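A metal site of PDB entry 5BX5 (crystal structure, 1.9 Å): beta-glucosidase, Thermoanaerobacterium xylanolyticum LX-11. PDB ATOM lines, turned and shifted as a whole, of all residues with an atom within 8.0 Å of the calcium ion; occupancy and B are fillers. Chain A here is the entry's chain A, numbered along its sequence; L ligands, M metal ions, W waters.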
ATOM      1  N   LYS A 557      32.954 -23.630 -16.714  1.00  0.00           N
ATOM      2  CA  LYS A 557      32.629 -22.934 -15.453  1.00  0.00           C
ATOM      3  C   LYS A 557      32.138 -21.510 -15.705  1.00  0.00           C
ATOM      4  O   LYS A 557      31.202 -21.055 -15.056  1.00  0.00           O
ATOM      5  CB  LYS A 557      33.849 -22.933 -14.521  1.00  0.00           C
ATOM      6  CG  LYS A 557      33.622 -22.445 -13.099  1.00  0.00           C
ATOM      7  CD  LYS A 557      32.424 -23.094 -12.442  1.00  0.00           C
ATOM      8  CE  LYS A 557      32.594 -23.255 -10.944  1.00  0.00           C
ATOM      9  NZ  LYS A 557      32.854 -21.986 -10.239  1.00  0.00           N
ATOM     10  N   MET A 559      30.245 -20.515 -17.884  1.00  0.00           N
ATOM     11  CA  MET A 559      28.840 -20.524 -18.312  1.00  0.00           C
ATOM     12  C   MET A 559      27.836 -20.652 -17.175  1.00  0.00           C
ATOM     13  O   MET A 559      26.614 -20.736 -17.400  1.00  0.00           O
ATOM     14  CB  MET A 559      28.642 -21.625 -19.353  1.00  0.00           C
ATOM     15  CG  MET A 559      29.389 -21.339 -20.634  1.00  0.00           C
ATOM     16  SD  MET A 559      29.296 -22.668 -21.838  1.00  0.00           S
ATOM     17  CE  MET A 559      30.340 -21.991 -23.136  1.00  0.00           C
ATOM     18  N   ASP A 560      28.329 -20.671 -15.947  1.00  0.00           N
ATOM     19  CA  ASP A 560      27.459 -20.644 -14.775  1.00  0.00           C
ATOM     20  C   ASP A 560      27.037 -19.194 -14.545  1.00  0.00           C
ATOM     21  O   ASP A 560      27.827 -18.405 -14.102  1.00  0.00           O
ATOM     22  CB  ASP A 560      28.235 -21.140 -13.560  1.00  0.00           C
ATOM     23  CG  ASP A 560      27.443 -21.037 -12.280  1.00  0.00           C
ATOM     24  OD1 ASP A 560      26.191 -20.926 -12.330  1.00  0.00           O
ATOM     25  OD2 ASP A 560      28.076 -21.072 -11.228  1.00  0.00           O
ATOM     26  N   LYS A 561      25.790 -18.864 -14.850  1.00  0.00           N
ATOM     27  CA  LYS A 561      25.343 -17.468 -14.808  1.00  0.00           C
ATOM     28  C   LYS A 561      24.895 -17.009 -13.427  1.00  0.00           C
ATOM     29  O   LYS A 561      24.920 -15.816 -13.137  1.00  0.00           O
ATOM     30  CB  LYS A 561      24.163 -17.266 -15.764  1.00  0.00           C
ATOM     31  CG  LYS A 561      24.506 -17.401 -17.244  1.00  0.00           C
ATOM     32  CD  LYS A 561      23.220 -17.665 -18.029  1.00  0.00           C
ATOM     33  CE  LYS A 561      23.393 -17.367 -19.506  1.00  0.00           C
ATOM     34  NZ  LYS A 561      22.086 -17.444 -20.234  1.00  0.00           N
ATOM     35  N   ASP A 562      24.493 -17.941 -12.573  1.00  0.00           N
ATOM     36  CA  ASP A 562      23.864 -17.550 -11.312  1.00  0.00           C
ATOM     37  C   ASP A 562      24.641 -18.043 -10.111  1.00  0.00           C
ATOM     38  O   ASP A 562      24.093 -18.150  -9.010  1.00  0.00           O
ATOM     39  CB  ASP A 562      22.442 -18.076 -11.271  1.00  0.00           C
ATOM     40  CG  ASP A 562      22.387 -19.583 -11.177  1.00  0.00           C
ATOM     41  OD1 ASP A 562      23.383 -20.247 -11.543  1.00  0.00           O
ATOM     42  OD2 ASP A 562      21.342 -20.087 -10.725  1.00  0.00           O
ATOM     43  N   ASN A 563      25.910 -18.321 -10.316  1.00  0.00           N
ATOM     44  CA  ASN A 563      26.812 -18.798  -9.279  1.00  0.00           C
ATOM     45  C   ASN A 563      26.274 -19.940  -8.372  1.00  0.00           C
ATOM     46  O   ASN A 563      26.496 -19.937  -7.167  1.00  0.00           O
ATOM     47  CB  ASN A 563      27.305 -17.609  -8.434  1.00  0.00           C
ATOM     48  CG  ASN A 563      28.597 -17.908  -7.676  1.00  0.00           C
ATOM     49  OD1 ASN A 563      29.509 -18.554  -8.196  1.00  0.00           O
ATOM     50  ND2 ASN A 563      28.663 -17.454  -6.435  1.00  0.00           N
ATOM     51  N   ASP A 564      25.576 -20.926  -8.942  1.00  0.00           N
ATOM     52  CA  ASP A 564      25.292 -22.167  -8.203  1.00  0.00           C
ATOM     53  C   ASP A 564      26.385 -23.232  -8.417  1.00  0.00           C
ATOM     54  O   ASP A 564      26.289 -24.349  -7.887  1.00  0.00           O
ATOM     55  CB  ASP A 564      23.888 -22.726  -8.532  1.00  0.00           C
ATOM     56  CG  ASP A 564      23.801 -23.368  -9.920  1.00  0.00           C
ATOM     57  OD1 ASP A 564      24.681 -23.116 -10.773  1.00  0.00           O
ATOM     58  OD2 ASP A 564      22.815 -24.100 -10.171  1.00  0.00           O
ATOM     59  N   GLY A 565      27.430 -22.876  -9.186  1.00  0.00           N
ATOM     60  CA  GLY A 565      28.570 -23.764  -9.436  1.00  0.00           C
ATOM     61  C   GLY A 565      28.396 -24.731 -10.613  1.00  0.00           C
ATOM     62  O   GLY A 565      29.250 -25.591 -10.836  1.00  0.00           O
ATOM     63  N   ILE A 566      27.285 -24.581 -11.344  1.00  0.00           N
ATOM     64  CA  ILE A 566      26.906 -25.470 -12.455  1.00  0.00           C
ATOM     65  C   ILE A 566      26.625 -24.621 -13.700  1.00  0.00           C
ATOM     66  O   ILE A 566      25.915 -23.605 -13.600  1.00  0.00           O
ATOM     67  CB  ILE A 566      25.636 -26.273 -12.085  1.00  0.00           C
ATOM     68  CG1 ILE A 566      25.838 -26.996 -10.743  1.00  0.00           C
ATOM     69  CG2 ILE A 566      25.253 -27.265 -13.191  1.00  0.00           C
ATOM     70  CD1 ILE A 566      24.603 -27.669 -10.202  1.00  0.00           C
ATOM     71  N   PRO A 567      27.170 -25.008 -14.870  1.00  0.00           N
ATOM     72  CA  PRO A 567      26.829 -24.278 -16.102  1.00  0.00           C
ATOM     73  C   PRO A 567      25.330 -24.252 -16.367  1.00  0.00           C
ATOM     74  O   PRO A 567      24.637 -25.234 -16.086  1.00  0.00           O
ATOM     75  CB  PRO A 567      27.585 -25.020 -17.212  1.00  0.00           C
ATOM     76  CG  PRO A 567      28.017 -26.320 -16.607  1.00  0.00           C
ATOM     77  CD  PRO A 567      28.057 -26.157 -15.115  1.00  0.00           C
ATOM     78  N   ASP A 568      24.832 -23.114 -16.852  1.00  0.00           N
ATOM     79  CA  ASP A 568      23.409 -22.943 -17.138  1.00  0.00           C
ATOM     80  C   ASP A 568      23.089 -23.284 -18.585  1.00  0.00           C
ATOM     81  O   ASP A 568      23.677 -22.712 -19.497  1.00  0.00           O
ATOM     82  CB  ASP A 568      22.986 -21.473 -16.918  1.00  0.00           C
ATOM     83  CG  ASP A 568      22.961 -21.064 -15.453  1.00  0.00           C
ATOM     84  OD1 ASP A 568      24.011 -21.173 -14.766  1.00  0.00           O
ATOM     85  OD2 ASP A 568      21.886 -20.599 -14.991  1.00  0.00           O
ATOM     86  N   ASN A 569      22.147 -24.217 -18.801  1.00  0.00           N
ATOM     87  CA  ASN A 569      21.564 -24.390 -20.122  1.00  0.00           C
ATOM     88  C   ASN A 569      20.753 -23.117 -20.434  1.00  0.00           C
ATOM     89  O   ASN A 569      20.112 -22.539 -19.559  1.00  0.00           O
ATOM     90  CB  ASN A 569      20.700 -25.662 -20.185  1.00  0.00           C
ATOM     91  CG  ASN A 569      21.515 -26.931 -19.996  1.00  0.00           C
ATOM     92  OD1 ASN A 569      21.601 -27.482 -18.898  1.00  0.00           O
ATOM     93  ND2 ASN A 569      22.123 -27.402 -21.067  1.00  0.00           N
ATOM     94  N   GLY A 584      18.556 -23.696 -17.389  1.00  0.00           N
ATOM     95  CA  GLY A 584      19.017 -23.691 -16.018  1.00  0.00           C
ATOM     96  C   GLY A 584      19.983 -24.824 -15.731  1.00  0.00           C
ATOM     97  O   GLY A 584      20.871 -25.103 -16.546  1.00  0.00           O
ATOM     98  N   THR A 585      19.824 -25.457 -14.578  1.00  0.00           N
ATOM     99  CA  THR A 585      20.569 -26.668 -14.248  1.00  0.00           C
ATOM    100  C   THR A 585      19.752 -27.852 -14.790  1.00  0.00           C
ATOM    101  O   THR A 585      18.579 -28.013 -14.448  1.00  0.00           O
ATOM    102  CB  THR A 585      20.806 -26.799 -12.732  1.00  0.00           C
ATOM    103  OG1 THR A 585      21.712 -25.782 -12.296  1.00  0.00           O
ATOM    104  CG2 THR A 585      21.402 -28.140 -12.397  1.00  0.00           C
ATOM    105  N   TRP A 593      28.692 -32.765 -15.711  1.00  0.00           N
ATOM    106  CA  TRP A 593      29.613 -31.804 -15.098  1.00  0.00           C
ATOM    107  C   TRP A 593      30.186 -32.322 -13.769  1.00  0.00           C
ATOM    108  O   TRP A 593      31.391 -32.250 -13.519  1.00  0.00           O
ATOM    109  CB  TRP A 593      28.844 -30.495 -14.898  1.00  0.00           C
ATOM    110  CG  TRP A 593      29.517 -29.386 -14.120  1.00  0.00           C
ATOM    111  CD1 TRP A 593      29.087 -28.852 -12.938  1.00  0.00           C
ATOM    112  CD2 TRP A 593      30.696 -28.658 -14.476  1.00  0.00           C
ATOM    113  NE1 TRP A 593      29.926 -27.844 -12.530  1.00  0.00           N
ATOM    114  CE2 TRP A 593      30.927 -27.711 -13.454  1.00  0.00           C
ATOM    115  CE3 TRP A 593      31.586 -28.723 -15.554  1.00  0.00           C
ATOM    116  CZ2 TRP A 593      32.006 -26.826 -13.482  1.00  0.00           C
ATOM    117  CZ3 TRP A 593      32.658 -27.849 -15.585  1.00  0.00           C
ATOM    118  CH2 TRP A 593      32.855 -26.901 -14.550  1.00  0.00           C
ATOM    119  N   ASN A 626      24.319 -28.358  -4.745  1.00  0.00           N
ATOM    120  CA  ASN A 626      23.290 -27.598  -5.448  1.00  0.00           C
ATOM    121  C   ASN A 626      22.487 -28.425  -6.460  1.00  0.00           C
ATOM    122  O   ASN A 626      21.298 -28.196  -6.618  1.00  0.00           O
ATOM    123  CB  ASN A 626      23.875 -26.341  -6.087  1.00  0.00           C
ATOM    124  CG  ASN A 626      24.235 -25.301  -5.043  1.00  0.00           C
ATOM    125  OD1 ASN A 626      23.609 -25.261  -3.986  1.00  0.00           O
ATOM    126  ND2 ASN A 626      25.202 -24.468  -5.322  1.00  0.00           N
ATOM    127  N   GLU A 630      18.461 -28.672  -6.163  1.00  0.00           N
ATOM    128  CA  GLU A 630      17.683 -28.136  -7.267  1.00  0.00           C
ATOM    129  C   GLU A 630      16.798 -29.163  -7.944  1.00  0.00           C
ATOM    130  O   GLU A 630      15.728 -28.826  -8.441  1.00  0.00           O
ATOM    131  CB  GLU A 630      18.622 -27.512  -8.308  1.00  0.00           C
ATOM    132  CG  GLU A 630      19.254 -26.193  -7.868  1.00  0.00           C
ATOM    133  CD  GLU A 630      20.446 -25.814  -8.719  1.00  0.00           C
ATOM    134  OE1 GLU A 630      20.635 -26.412  -9.797  1.00  0.00           O
ATOM    135  OE2 GLU A 630      21.215 -24.924  -8.283  1.00  0.00           O
ATOM    136  N   THR A 641      15.680 -27.087 -14.155  1.00  0.00           N
ATOM    137  CA  THR A 641      15.124 -26.174 -13.162  1.00  0.00           C
ATOM    138  C   THR A 641      14.200 -25.088 -13.726  1.00  0.00           C
ATOM    139  O   THR A 641      13.462 -24.480 -12.959  1.00  0.00           O
ATOM    140  CB  THR A 641      16.248 -25.485 -12.361  1.00  0.00           C
ATOM    141  OG1 THR A 641      17.151 -24.823 -13.264  1.00  0.00           O
ATOM    142  CG2 THR A 641      17.001 -26.487 -11.511  1.00  0.00           C
ATOM    143  N   GLU A 642      14.217 -24.838 -15.034  1.00  0.00           N
ATOM    144  CA  GLU A 642      13.494 -23.674 -15.598  1.00  0.00           C
ATOM    145  C   GLU A 642      12.584 -23.916 -16.815  1.00  0.00           C
ATOM    146  O   GLU A 642      11.818 -23.022 -17.190  1.00  0.00           O
ATOM    147  CB  GLU A 642      14.480 -22.535 -15.907  1.00  0.00           C
ATOM    148  CG  GLU A 642      15.227 -22.005 -14.676  1.00  0.00           C
ATOM    149  CD  GLU A 642      16.234 -20.904 -15.022  1.00  0.00           C
ATOM    150  OE1 GLU A 642      15.998 -20.154 -15.996  1.00  0.00           O
ATOM    151  OE2 GLU A 642      17.259 -20.787 -14.321  1.00  0.00           O
HETATM  152  C1  LIG L   1      19.328 -23.313 -10.538  1.00  0.00           C
HETATM  153  O1  LIG L   1      18.269 -23.239  -9.576  1.00  0.00           O
HETATM  154  C2  LIG L   1      19.133 -22.249 -11.626  1.00  0.00           C
HETATM  155  O2  LIG L   1      17.881 -22.456 -12.288  1.00  0.00           O
HETATM  156  C3  LIG L   1      20.242 -22.289 -12.672  1.00  0.00           C
HETATM  157  O3  LIG L   1      21.541 -22.493 -12.095  1.00  0.00           O
HETATM  158 CA    CA M   1      24.306 -22.214 -12.802  1.00  0.00          CA
HETATM  159  O   HOH W   1      23.022 -24.050 -13.745  1.00  0.00           O
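The backbone NH (N) of Asn 563 lies close to the side-chain carboxylate (OD1) of Asp 560 (3.3 Å).
O of Asp 564 lies within hydrogen-bond range of ND2 of Asn 626, at 2.8 Å.
OD2 of Asp 560 sits at hydrogen-bond distance from N of Gly 565 (2.8 Å).
OD1 of Asp 568 sits close to N of Lys 561, at 2.9 Å.
The side-chain carboxylate of Asp 564 sits at hydrogen-bond distance from the side-chain hydroxyl of Thr 585, 2.9 Å away.
OD2 of Asp 564 lies close to OE2 of Glu 630 (2.6 Å).
The backbone NH (N) of Asp 568 is in hydrogen-bond range of the backbone carbonyl oxygen (O) of Met 559, 3.0 Å away.
The nearest printed residue that does not touch the calcium ion is Lys 561 (4.2 Å).
The calcium ion is bound by the side-chain carboxylate of Asp 568, the side-chain carboxylate of Asp 564, the backbone carbonyl oxygen of Ile 566, the side-chain carboxylate of Asp 560, water W1, the side-chain carboxylate of Asp 562 and an oxygen (O3) of the ligand.
Water W1 bridges the side-chain hydroxyl of Thr 585 (2.6 Å) and the backbone carbonyl oxygen of Pro 567 (3.1 Å).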
